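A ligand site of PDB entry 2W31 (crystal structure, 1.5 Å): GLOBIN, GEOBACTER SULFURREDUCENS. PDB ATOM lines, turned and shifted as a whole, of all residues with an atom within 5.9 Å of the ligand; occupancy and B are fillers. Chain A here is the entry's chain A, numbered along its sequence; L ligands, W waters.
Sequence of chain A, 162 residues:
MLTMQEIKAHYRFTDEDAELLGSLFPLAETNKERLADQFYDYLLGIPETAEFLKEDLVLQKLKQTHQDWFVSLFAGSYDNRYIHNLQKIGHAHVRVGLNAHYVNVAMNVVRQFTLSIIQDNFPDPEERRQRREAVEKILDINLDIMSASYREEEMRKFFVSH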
ATOM      1  N   PHE A  39      -3.711  -8.362  26.192  1.00  0.00           N
ATOM      2  CA  PHE A  39      -4.629  -7.418  26.820  1.00  0.00           C
ATOM      3  C   PHE A  39      -5.064  -7.924  28.197  1.00  0.00           C
ATOM      4  O   PHE A  39      -4.923  -7.220  29.213  1.00  0.00           O
ATOM      5  CB  PHE A  39      -5.838  -7.193  25.871  1.00  0.00           C
ATOM      6  CG  PHE A  39      -6.836  -6.199  26.347  1.00  0.00           C
ATOM      7  CD1 PHE A  39      -6.752  -4.871  25.955  1.00  0.00           C
ATOM      8  CD2 PHE A  39      -7.943  -6.593  27.109  1.00  0.00           C
ATOM      9  CE1 PHE A  39      -7.721  -3.946  26.349  1.00  0.00           C
ATOM     10  CE2 PHE A  39      -8.925  -5.679  27.503  1.00  0.00           C
ATOM     11  CZ  PHE A  39      -8.805  -4.339  27.111  1.00  0.00           C
ATOM     12  N   LEU A  43      -3.946  -6.628  32.221  1.00  0.00           N
ATOM     13  CA  LEU A  43      -4.920  -6.241  33.247  1.00  0.00           C
ATOM     14  C   LEU A  43      -4.773  -7.049  34.533  1.00  0.00           C
ATOM     15  O   LEU A  43      -4.938  -6.496  35.644  1.00  0.00           O
ATOM     16  CB  LEU A  43      -6.343  -6.345  32.697  1.00  0.00           C
ATOM     17  CG  LEU A  43      -6.714  -5.411  31.530  1.00  0.00           C
ATOM     18  CD1 LEU A  43      -8.177  -5.594  31.124  1.00  0.00           C
ATOM     19  CD2 LEU A  43      -6.417  -3.955  31.871  1.00  0.00           C
ATOM     20  N   THR A  49      -7.503  -3.473  38.255  1.00  0.00           N
ATOM     21  CA  THR A  49      -8.236  -4.082  37.139  1.00  0.00           C
ATOM     22  C   THR A  49      -8.322  -5.610  37.357  1.00  0.00           C
ATOM     23  O   THR A  49      -9.299  -6.207  36.936  1.00  0.00           O
ATOM     24  CB  THR A  49      -7.581  -3.778  35.789  1.00  0.00           C
ATOM     25  OG1 THR A  49      -6.161  -4.028  35.871  1.00  0.00           O
ATOM     26  CG2 THR A  49      -7.823  -2.328  35.438  1.00  0.00           C
ATOM     27  N   ALA A  50      -7.328  -6.202  38.014  1.00  0.00           N
ATOM     28  CA  ALA A  50      -7.323  -7.642  38.253  1.00  0.00           C
ATOM     29  C   ALA A  50      -8.573  -8.056  39.050  1.00  0.00           C
ATOM     30  O   ALA A  50      -9.087  -9.173  38.886  1.00  0.00           O
ATOM     31  CB  ALA A  50      -6.034  -8.099  38.950  1.00  0.00           C
ATOM     32  N   PHE A  52     -11.624  -7.088  38.671  1.00  0.00           N
ATOM     33  CA  PHE A  52     -12.796  -7.260  37.814  1.00  0.00           C
ATOM     34  C   PHE A  52     -12.745  -8.542  37.065  1.00  0.00           C
ATOM     35  O   PHE A  52     -13.744  -8.908  36.451  1.00  0.00           O
ATOM     36  CB  PHE A  52     -12.919  -6.119  36.776  1.00  0.00           C
ATOM     37  CG  PHE A  52     -13.270  -4.798  37.383  1.00  0.00           C
ATOM     38  CD1 PHE A  52     -14.624  -4.423  37.527  1.00  0.00           C
ATOM     39  CD2 PHE A  52     -12.286  -3.962  37.872  1.00  0.00           C
ATOM     40  CE1 PHE A  52     -14.954  -3.206  38.123  1.00  0.00           C
ATOM     41  CE2 PHE A  52     -12.608  -2.719  38.476  1.00  0.00           C
ATOM     42  CZ  PHE A  52     -13.957  -2.368  38.616  1.00  0.00           C
ATOM     43  N   LEU A  53     -11.594  -9.221  37.084  1.00  0.00           N
ATOM     44  CA  LEU A  53     -11.410 -10.473  36.347  1.00  0.00           C
ATOM     45  C   LEU A  53     -11.475 -11.713  37.225  1.00  0.00           C
ATOM     46  O   LEU A  53     -11.247 -12.830  36.709  1.00  0.00           O
ATOM     47  CB  LEU A  53     -10.097 -10.433  35.593  1.00  0.00           C
ATOM     48  CG  LEU A  53     -10.032  -9.279  34.573  1.00  0.00           C
ATOM     49  CD1 LEU A  53      -8.708  -9.360  33.893  1.00  0.00           C
ATOM     50  CD2 LEU A  53     -11.183  -9.360  33.553  1.00  0.00           C
ATOM     51  N   LEU A  62     -14.908 -12.636  29.456  1.00  0.00           N
ATOM     52  CA  LEU A  62     -14.406 -11.272  29.195  1.00  0.00           C
ATOM     53  C   LEU A  62     -13.234 -11.190  28.202  1.00  0.00           C
ATOM     54  O   LEU A  62     -13.142 -10.195  27.485  1.00  0.00           O
ATOM     55  CB  LEU A  62     -14.068 -10.525  30.490  1.00  0.00           C
ATOM     56  CG  LEU A  62     -15.277 -10.147  31.361  1.00  0.00           C
ATOM     57  CD1 LEU A  62     -14.837  -9.563  32.678  1.00  0.00           C
ATOM     58  CD2 LEU A  62     -16.241  -9.148  30.633  1.00  0.00           C
ATOM     59  N   THR A  65     -15.053 -11.176  24.950  1.00  0.00           N
ATOM     60  CA  THR A  65     -15.766  -9.916  24.762  1.00  0.00           C
ATOM     61  C   THR A  65     -14.847  -8.785  24.257  1.00  0.00           C
ATOM     62  O   THR A  65     -15.197  -8.044  23.315  1.00  0.00           O
ATOM     63  CB  THR A  65     -16.426  -9.497  26.084  1.00  0.00           C
ATOM     64  OG1 THR A  65     -17.478 -10.419  26.379  1.00  0.00           O
ATOM     65  CG2 THR A  65     -17.022  -8.116  25.987  1.00  0.00           C
ATOM     66  N   HIS A  66     -13.661  -8.679  24.844  1.00  0.00           N
ATOM     67  CA  HIS A  66     -12.728  -7.627  24.429  1.00  0.00           C
ATOM     68  C   HIS A  66     -12.033  -8.006  23.095  1.00  0.00           C
ATOM     69  O   HIS A  66     -11.753  -7.104  22.261  1.00  0.00           O
ATOM     70  CB  HIS A  66     -11.759  -7.327  25.553  1.00  0.00           C
ATOM     71  CG  HIS A  66     -12.437  -6.702  26.727  1.00  0.00           C
ATOM     72  ND1 HIS A  66     -13.062  -7.443  27.716  1.00  0.00           N
ATOM     73  CD2 HIS A  66     -12.654  -5.409  27.047  1.00  0.00           C
ATOM     74  CE1 HIS A  66     -13.621  -6.625  28.580  1.00  0.00           C
ATOM     75  NE2 HIS A  66     -13.338  -5.377  28.219  1.00  0.00           N
ATOM     76  N   TRP A  69     -14.465  -6.880  20.366  1.00  0.00           N
ATOM     77  CA  TRP A  69     -14.399  -5.425  20.182  1.00  0.00           C
ATOM     78  C   TRP A  69     -13.188  -5.036  19.282  1.00  0.00           C
ATOM     79  O   TRP A  69     -13.304  -4.196  18.355  1.00  0.00           O
ATOM     80  CB  TRP A  69     -14.326  -4.682  21.531  1.00  0.00           C
ATOM     81  CG  TRP A  69     -13.880  -3.226  21.330  1.00  0.00           C
ATOM     82  CD1 TRP A  69     -14.648  -2.156  20.966  1.00  0.00           C
ATOM     83  CD2 TRP A  69     -12.516  -2.739  21.391  1.00  0.00           C
ATOM     84  NE1 TRP A  69     -13.836  -1.019  20.795  1.00  0.00           N
ATOM     85  CE2 TRP A  69     -12.537  -1.360  21.067  1.00  0.00           C
ATOM     86  CE3 TRP A  69     -11.277  -3.347  21.709  1.00  0.00           C
ATOM     87  CZ2 TRP A  69     -11.363  -0.582  21.056  1.00  0.00           C
ATOM     88  CZ3 TRP A  69     -10.125  -2.587  21.705  1.00  0.00           C
ATOM     89  CH2 TRP A  69     -10.182  -1.202  21.373  1.00  0.00           C
ATOM     90  N   ASN A  85     -23.345   2.198  19.858  1.00  0.00           N
ATOM     91  CA  ASN A  85     -22.774   1.027  20.493  1.00  0.00           C
ATOM     92  C   ASN A  85     -21.575   1.363  21.395  1.00  0.00           C
ATOM     93  O   ASN A  85     -21.446   0.797  22.492  1.00  0.00           O
ATOM     94  CB  ASN A  85     -22.386  -0.015  19.456  1.00  0.00           C
ATOM     95  CG  ASN A  85     -22.088  -1.329  20.081  1.00  0.00           C
ATOM     96  OD1 ASN A  85     -22.956  -1.919  20.736  1.00  0.00           O
ATOM     97  ND2 ASN A  85     -20.862  -1.786  19.932  1.00  0.00           N
ATOM     98  N   LYS A  88     -22.747   2.747  24.610  1.00  0.00           N
ATOM     99  CA  LYS A  88     -23.195   1.624  25.451  1.00  0.00           C
ATOM    100  C   LYS A  88     -22.021   0.956  26.148  1.00  0.00           C
ATOM    101  O   LYS A  88     -22.079   0.660  27.365  1.00  0.00           O
ATOM    102  CB  LYS A  88     -23.927   0.589  24.582  1.00  0.00           C
ATOM    103  CG  LYS A  88     -24.338  -0.699  25.273  1.00  0.00           C
ATOM    104  CD  LYS A  88     -25.158  -1.606  24.353  1.00  0.00           C
ATOM    105  CE  LYS A  88     -25.361  -2.968  24.993  1.00  0.00           C
ATOM    106  NZ  LYS A  88     -25.111  -4.044  23.984  1.00  0.00           N
ATOM    107  N   ILE A  89     -20.951   0.748  25.392  1.00  0.00           N
ATOM    108  CA  ILE A  89     -19.732   0.126  25.922  1.00  0.00           C
ATOM    109  C   ILE A  89     -19.190   1.000  27.051  1.00  0.00           C
ATOM    110  O   ILE A  89     -18.839   0.522  28.114  1.00  0.00           O
ATOM    111  CB  ILE A  89     -18.662  -0.115  24.803  1.00  0.00           C
ATOM    112  CG1 ILE A  89     -19.174  -1.139  23.777  1.00  0.00           C
ATOM    113  CG2 ILE A  89     -17.358  -0.616  25.403  1.00  0.00           C
ATOM    114  CD1 ILE A  89     -18.486  -1.077  22.400  1.00  0.00           C
ATOM    115  N   ALA A  92     -21.240   0.636  30.256  1.00  0.00           N
ATOM    116  CA  ALA A  92     -21.060  -0.666  30.913  1.00  0.00           C
ATOM    117  C   ALA A  92     -19.927  -0.581  31.941  1.00  0.00           C
ATOM    118  O   ALA A  92     -20.027  -1.129  33.040  1.00  0.00           O
ATOM    119  CB  ALA A  92     -20.760  -1.738  29.887  1.00  0.00           C
ATOM    120  N   HIS A  93     -18.851   0.146  31.578  1.00  0.00           N
ATOM    121  CA  HIS A  93     -17.714   0.279  32.471  1.00  0.00           C
ATOM    122  C   HIS A  93     -18.021   1.235  33.652  1.00  0.00           C
ATOM    123  O   HIS A  93     -17.583   0.983  34.772  1.00  0.00           O
ATOM    124  CB  HIS A  93     -16.423   0.654  31.683  1.00  0.00           C
ATOM    125  CG  HIS A  93     -15.996  -0.391  30.687  1.00  0.00           C
ATOM    126  ND1 HIS A  93     -16.482  -0.426  29.396  1.00  0.00           N
ATOM    127  CD2 HIS A  93     -15.122  -1.439  30.778  1.00  0.00           C
ATOM    128  CE1 HIS A  93     -15.965  -1.445  28.744  1.00  0.00           C
ATOM    129  NE2 HIS A  93     -15.115  -2.074  29.543  1.00  0.00           N
ATOM    130  N   ARG A  95     -20.997   1.607  34.914  1.00  0.00           N
ATOM    131  CA  ARG A  95     -21.914   0.807  35.740  1.00  0.00           C
ATOM    132  C   ARG A  95     -21.217  -0.185  36.690  1.00  0.00           C
ATOM    133  O   ARG A  95     -21.636  -0.354  37.842  1.00  0.00           O
ATOM    134  CB  ARG A  95     -22.888   0.096  34.798  1.00  0.00           C
ATOM    135  CG  ARG A  95     -23.703  -1.058  35.369  1.00  0.00           C
ATOM    136  CD  ARG A  95     -24.295  -1.883  34.207  1.00  0.00           C
ATOM    137  NE  ARG A  95     -24.787  -1.004  33.141  1.00  0.00           N
ATOM    138  CZ  ARG A  95     -24.699  -1.262  31.836  1.00  0.00           C
ATOM    139  NH1 ARG A  95     -24.136  -2.380  31.402  1.00  0.00           N
ATOM    140  NH2 ARG A  95     -25.179  -0.380  30.970  1.00  0.00           N
ATOM    141  N   VAL A  96     -20.152  -0.841  36.230  1.00  0.00           N
ATOM    142  CA  VAL A  96     -19.446  -1.818  37.095  1.00  0.00           C
ATOM    143  C   VAL A  96     -18.408  -1.199  38.046  1.00  0.00           C
ATOM    144  O   VAL A  96     -17.815  -1.910  38.872  1.00  0.00           O
ATOM    145  CB  VAL A  96     -18.784  -2.967  36.294  1.00  0.00           C
ATOM    146  CG1 VAL A  96     -19.843  -3.704  35.494  1.00  0.00           C
ATOM    147  CG2 VAL A  96     -17.626  -2.446  35.398  1.00  0.00           C
ATOM    148  N   LEU A  98     -15.608   0.681  37.162  1.00  0.00           N
ATOM    149  CA  LEU A  98     -14.238   0.829  36.645  1.00  0.00           C
ATOM    150  C   LEU A  98     -13.870   2.330  36.475  1.00  0.00           C
ATOM    151  O   LEU A  98     -14.586   3.105  35.820  1.00  0.00           O
ATOM    152  CB  LEU A  98     -14.137   0.096  35.310  1.00  0.00           C
ATOM    153  CG  LEU A  98     -12.734   0.074  34.683  1.00  0.00           C
ATOM    154  CD1 LEU A  98     -11.754  -0.741  35.526  1.00  0.00           C
ATOM    155  CD2 LEU A  98     -12.818  -0.418  33.235  1.00  0.00           C
ATOM    156  N   TYR A 102      -8.429   3.542  33.715  1.00  0.00           N
ATOM    157  CA  TYR A 102      -8.039   2.210  33.226  1.00  0.00           C
ATOM    158  C   TYR A 102      -8.474   1.984  31.777  1.00  0.00           C
ATOM    159  O   TYR A 102      -7.841   1.185  31.072  1.00  0.00           O
ATOM    160  CB  TYR A 102      -8.529   1.108  34.164  1.00  0.00           C
ATOM    161  CG  TYR A 102      -7.876   1.250  35.514  1.00  0.00           C
ATOM    162  CD1 TYR A 102      -6.484   1.006  35.680  1.00  0.00           C
ATOM    163  CD2 TYR A 102      -8.602   1.703  36.623  1.00  0.00           C
ATOM    164  CE1 TYR A 102      -5.857   1.179  36.907  1.00  0.00           C
ATOM    165  CE2 TYR A 102      -7.980   1.891  37.882  1.00  0.00           C
ATOM    166  CZ  TYR A 102      -6.601   1.626  38.004  1.00  0.00           C
ATOM    167  OH  TYR A 102      -5.947   1.804  39.239  1.00  0.00           O
ATOM    168  N   VAL A 103      -9.505   2.714  31.330  1.00  0.00           N
ATOM    169  CA  VAL A 103      -9.884   2.696  29.902  1.00  0.00           C
ATOM    170  C   VAL A 103      -8.756   3.340  29.086  1.00  0.00           C
ATOM    171  O   VAL A 103      -8.328   2.799  28.039  1.00  0.00           O
ATOM    172  CB  VAL A 103     -11.290   3.365  29.631  1.00  0.00           C
ATOM    173  CG1 VAL A 103     -11.595   3.447  28.129  1.00  0.00           C
ATOM    174  CG2 VAL A 103     -12.403   2.554  30.321  1.00  0.00           C
ATOM    175  N   ALA A 106      -5.874   0.830  29.098  1.00  0.00           N
ATOM    176  CA  ALA A 106      -6.129  -0.307  28.222  1.00  0.00           C
ATOM    177  C   ALA A 106      -5.955   0.076  26.756  1.00  0.00           C
ATOM    178  O   ALA A 106      -5.495  -0.742  25.944  1.00  0.00           O
ATOM    179  CB  ALA A 106      -7.526  -0.856  28.462  1.00  0.00           C
ATOM    180  N   MET A 107      -6.307   1.309  26.417  1.00  0.00           N
ATOM    181  CA  MET A 107      -6.296   1.759  25.031  1.00  0.00           C
ATOM    182  C   MET A 107      -4.869   1.974  24.539  1.00  0.00           C
ATOM    183  O   MET A 107      -4.585   1.840  23.355  1.00  0.00           O
ATOM    184  CB  MET A 107      -7.107   3.046  24.883  1.00  0.00           C
ATOM    185  CG  MET A 107      -7.363   3.451  23.438  1.00  0.00           C
ATOM    186  SD  MET A 107      -8.295   2.205  22.526  1.00  0.00           S
ATOM    187  CE  MET A 107      -9.967   2.610  23.018  1.00  0.00           C
ATOM    188  N   VAL A 110      -3.711  -1.561  23.463  1.00  0.00           N
ATOM    189  CA  VAL A 110      -4.189  -1.897  22.112  1.00  0.00           C
ATOM    190  C   VAL A 110      -3.407  -1.106  21.055  1.00  0.00           C
ATOM    191  O   VAL A 110      -3.047  -1.621  19.971  1.00  0.00           O
ATOM    192  CB  VAL A 110      -5.708  -1.621  22.021  1.00  0.00           C
ATOM    193  CG1 VAL A 110      -6.254  -1.877  20.633  1.00  0.00           C
ATOM    194  CG2 VAL A 110      -6.447  -2.460  23.066  1.00  0.00           C
ATOM    195  N   ASN A 142     -12.697   5.839  19.396  1.00  0.00           N
ATOM    196  CA  ASN A 142     -13.228   4.927  20.415  1.00  0.00           C
ATOM    197  C   ASN A 142     -13.029   5.471  21.827  1.00  0.00           C
ATOM    198  O   ASN A 142     -13.943   5.507  22.654  1.00  0.00           O
ATOM    199  CB  ASN A 142     -12.629   3.527  20.251  1.00  0.00           C
ATOM    200  CG  ASN A 142     -13.379   2.680  19.217  1.00  0.00           C
ATOM    201  OD1 ASN A 142     -14.018   1.676  19.603  1.00  0.00           O
ATOM    202  ND2 ASN A 142     -13.341   3.080  17.963  1.00  0.00           N
ATOM    203  N   MET A 146     -16.017   6.720  24.494  1.00  0.00           N
ATOM    204  CA  MET A 146     -16.056   6.031  25.786  1.00  0.00           C
ATOM    205  C   MET A 146     -15.826   7.001  26.948  1.00  0.00           C
ATOM    206  O   MET A 146     -16.497   6.903  28.003  1.00  0.00           O
ATOM    207  CB  MET A 146     -15.055   4.878  25.834  1.00  0.00           C
ATOM    208  CG  MET A 146     -15.434   3.681  24.953  1.00  0.00           C
ATOM    209  SD  MET A 146     -14.315   2.294  25.133  1.00  0.00           S
ATOM    210  CE  MET A 146     -14.655   1.658  26.777  1.00  0.00           C
HETATM  211  C1  LIG L   1     -17.382  -4.932  29.090  1.00  0.00           C
HETATM  212  C2  LIG L   1     -14.668  -3.010  25.608  1.00  0.00           C
HETATM  213  C3  LIG L   1     -11.436  -1.728  28.984  1.00  0.00           C
HETATM  214  C4  LIG L   1     -13.551  -4.773  32.089  1.00  0.00           C
HETATM  215  C5  LIG L   1     -16.946  -4.516  27.852  1.00  0.00           C
HETATM  216  C6  LIG L   1     -17.673  -4.636  26.603  1.00  0.00           C
HETATM  217  C7  LIG L   1     -16.916  -4.126  25.629  1.00  0.00           C
HETATM  218  C8  LIG L   1     -15.691  -3.650  26.257  1.00  0.00           C
HETATM  219  C9  LIG L   1     -17.221  -4.017  24.115  1.00  0.00           C
HETATM  220  C10 LIG L   1     -19.099  -5.252  26.452  1.00  0.00           C
HETATM  221  C11 LIG L   1     -20.034  -4.137  26.948  1.00  0.00           C
HETATM  222  C12 LIG L   1     -21.489  -4.295  26.550  1.00  0.00           C
HETATM  223  O1  LIG L   1     -21.829  -4.147  25.341  1.00  0.00           O
HETATM  224  O2  LIG L   1     -22.310  -4.553  27.477  1.00  0.00           O
HETATM  225  C13 LIG L   1     -13.619  -2.367  26.249  1.00  0.00           C
HETATM  226  C14 LIG L   1     -12.676  -1.431  25.651  1.00  0.00           C
HETATM  227  C15 LIG L   1     -11.778  -1.083  26.569  1.00  0.00           C
HETATM  228  C16 LIG L   1     -12.097  -1.810  27.794  1.00  0.00           C
HETATM  229  C17 LIG L   1     -12.794  -0.982  24.174  1.00  0.00           C
HETATM  230  C18 LIG L   1     -10.581  -0.136  26.443  1.00  0.00           C
HETATM  231  C19 LIG L   1      -9.791  -0.141  25.349  1.00  0.00           C
HETATM  232  C20 LIG L   1     -11.673  -2.506  30.091  1.00  0.00           C
HETATM  233  C21 LIG L   1     -10.827  -2.630  31.256  1.00  0.00           C
HETATM  234  C22 LIG L   1     -11.394  -3.491  32.099  1.00  0.00           C
HETATM  235  C23 LIG L   1     -12.642  -3.931  31.503  1.00  0.00           C
HETATM  236  C24 LIG L   1      -9.493  -1.906  31.479  1.00  0.00           C
HETATM  237  C25 LIG L   1     -10.833  -3.923  33.470  1.00  0.00           C
HETATM  238  C26 LIG L   1     -10.650  -5.190  33.840  1.00  0.00           C
HETATM  239  C27 LIG L   1     -14.825  -4.981  31.619  1.00  0.00           C
HETATM  240  C28 LIG L   1     -15.917  -5.596  32.402  1.00  0.00           C
HETATM  241  C29 LIG L   1     -17.119  -5.645  31.480  1.00  0.00           C
HETATM  242  C30 LIG L   1     -16.633  -5.075  30.217  1.00  0.00           C
HETATM  243  C31 LIG L   1     -15.844  -6.046  33.854  1.00  0.00           C
HETATM  244  C32 LIG L   1     -18.533  -6.217  31.765  1.00  0.00           C
HETATM  245  C33 LIG L   1     -19.386  -5.261  32.585  1.00  0.00           C
HETATM  246  C34 LIG L   1     -20.579  -6.040  33.107  1.00  0.00           C
HETATM  247  O3  LIG L   1     -20.403  -7.037  33.855  1.00  0.00           O
HETATM  248  O4  LIG L   1     -21.713  -5.651  32.763  1.00  0.00           O
HETATM  249  N1  LIG L   1     -15.725  -3.914  27.617  1.00  0.00           N
HETATM  250  N2  LIG L   1     -13.238  -2.563  27.544  1.00  0.00           N
HETATM  251  N3  LIG L   1     -12.784  -3.323  30.258  1.00  0.00           N
HETATM  252  N4  LIG L   1     -15.307  -4.704  30.364  1.00  0.00           N
HETATM  253 FE1  LIG L   1     -14.248  -3.631  28.946  1.00  0.00          FE
HETATM  254  O   HOH W   1     -24.745  -2.696  28.743  1.00  0.00           O
HETATM  255  O   HOH W   2     -16.272  -7.281  36.970  1.00  0.00           O
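NZ of Lys 88 is in salt-bridge range of O1 of the ligand (3.6 Å).
An iron atom (FE1) of the ligand is bound by a ring nitrogen (NE2) of His 93 (1.9 Å).
A ring nitrogen (NE2) of His 66 is bound to an iron atom (FE1) of the ligand, 2.1 Å away.
ND1 of His 93 is in hydrogen-bond range of O of Ile 89 (2.8 Å).
The backbone carbonyl oxygen (O) of Leu 43 lies within hydrogen-bond range of the side-chain hydroxyl (OG1) of Thr 49.
O of Leu 43 is in hydrogen-bond range of N of Ala 50 (3.4 Å).
OD1 of Asn 142 sits at hydrogen-bond distance from NE1 of Trp 69 (3.0 Å).
N of Leu 98 lies within hydrogen-bond range of O of His 93.
A ring nitrogen (ND1) of His 66 is in hydrogen-bond range of the backbone carbonyl oxygen (O) of Leu 62 (2.8 Å).
Leu 43 touches the ligand (CD1 to C26, 3.7 Å).
O of Thr 49 touches C26 of the ligand, at 3.5 Å.
Phe 52 touches the ligand.
Leu 62 touches the ligand.
Thr 65 touches the ligand.
Trp 69 touches the ligand.
CG1 of Ile 89 touches C9 of the ligand, 3.5 Å away.
CB of Ala 92 touches C11 of the ligand (3.9 Å).
CG1 of Val 96 touches C33 of the ligand, at 3.3 Å.
Leu 98 touches the ligand (CD2 to C22, 3.6 Å).
Tyr 102 touches the ligand (O to C24, 3.5 Å).
CB of Ala 106 touches C18 of the ligand, 3.7 Å away.
CE of Met 107 touches C19 of the ligand (3.6 Å).
SD of Met 146 touches C17 of the ligand (3.7 Å).
Hydrophobic or aromatic side chains that line the ligand: Leu 43, Phe 52, Leu 62, His 66, Trp 69, Ile 89, Ala 92, His 93, Val 96, Leu 98, Ala 106, Met 107 and Met 146.
17 residues have an atom within 4 Å of the ligand: Leu 43, Thr 49, Phe 52, Leu 62, Thr 65, His 66, Trp 69, Lys 88, Ile 89, Ala 92, His 93, Val 96, Leu 98, Tyr 102, Ala 106, Met 107 and Met 146.
Water W1 lies within hydrogen-bond range of the guanidinium group of Arg 95 and an oxygen (O2) of the ligand.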
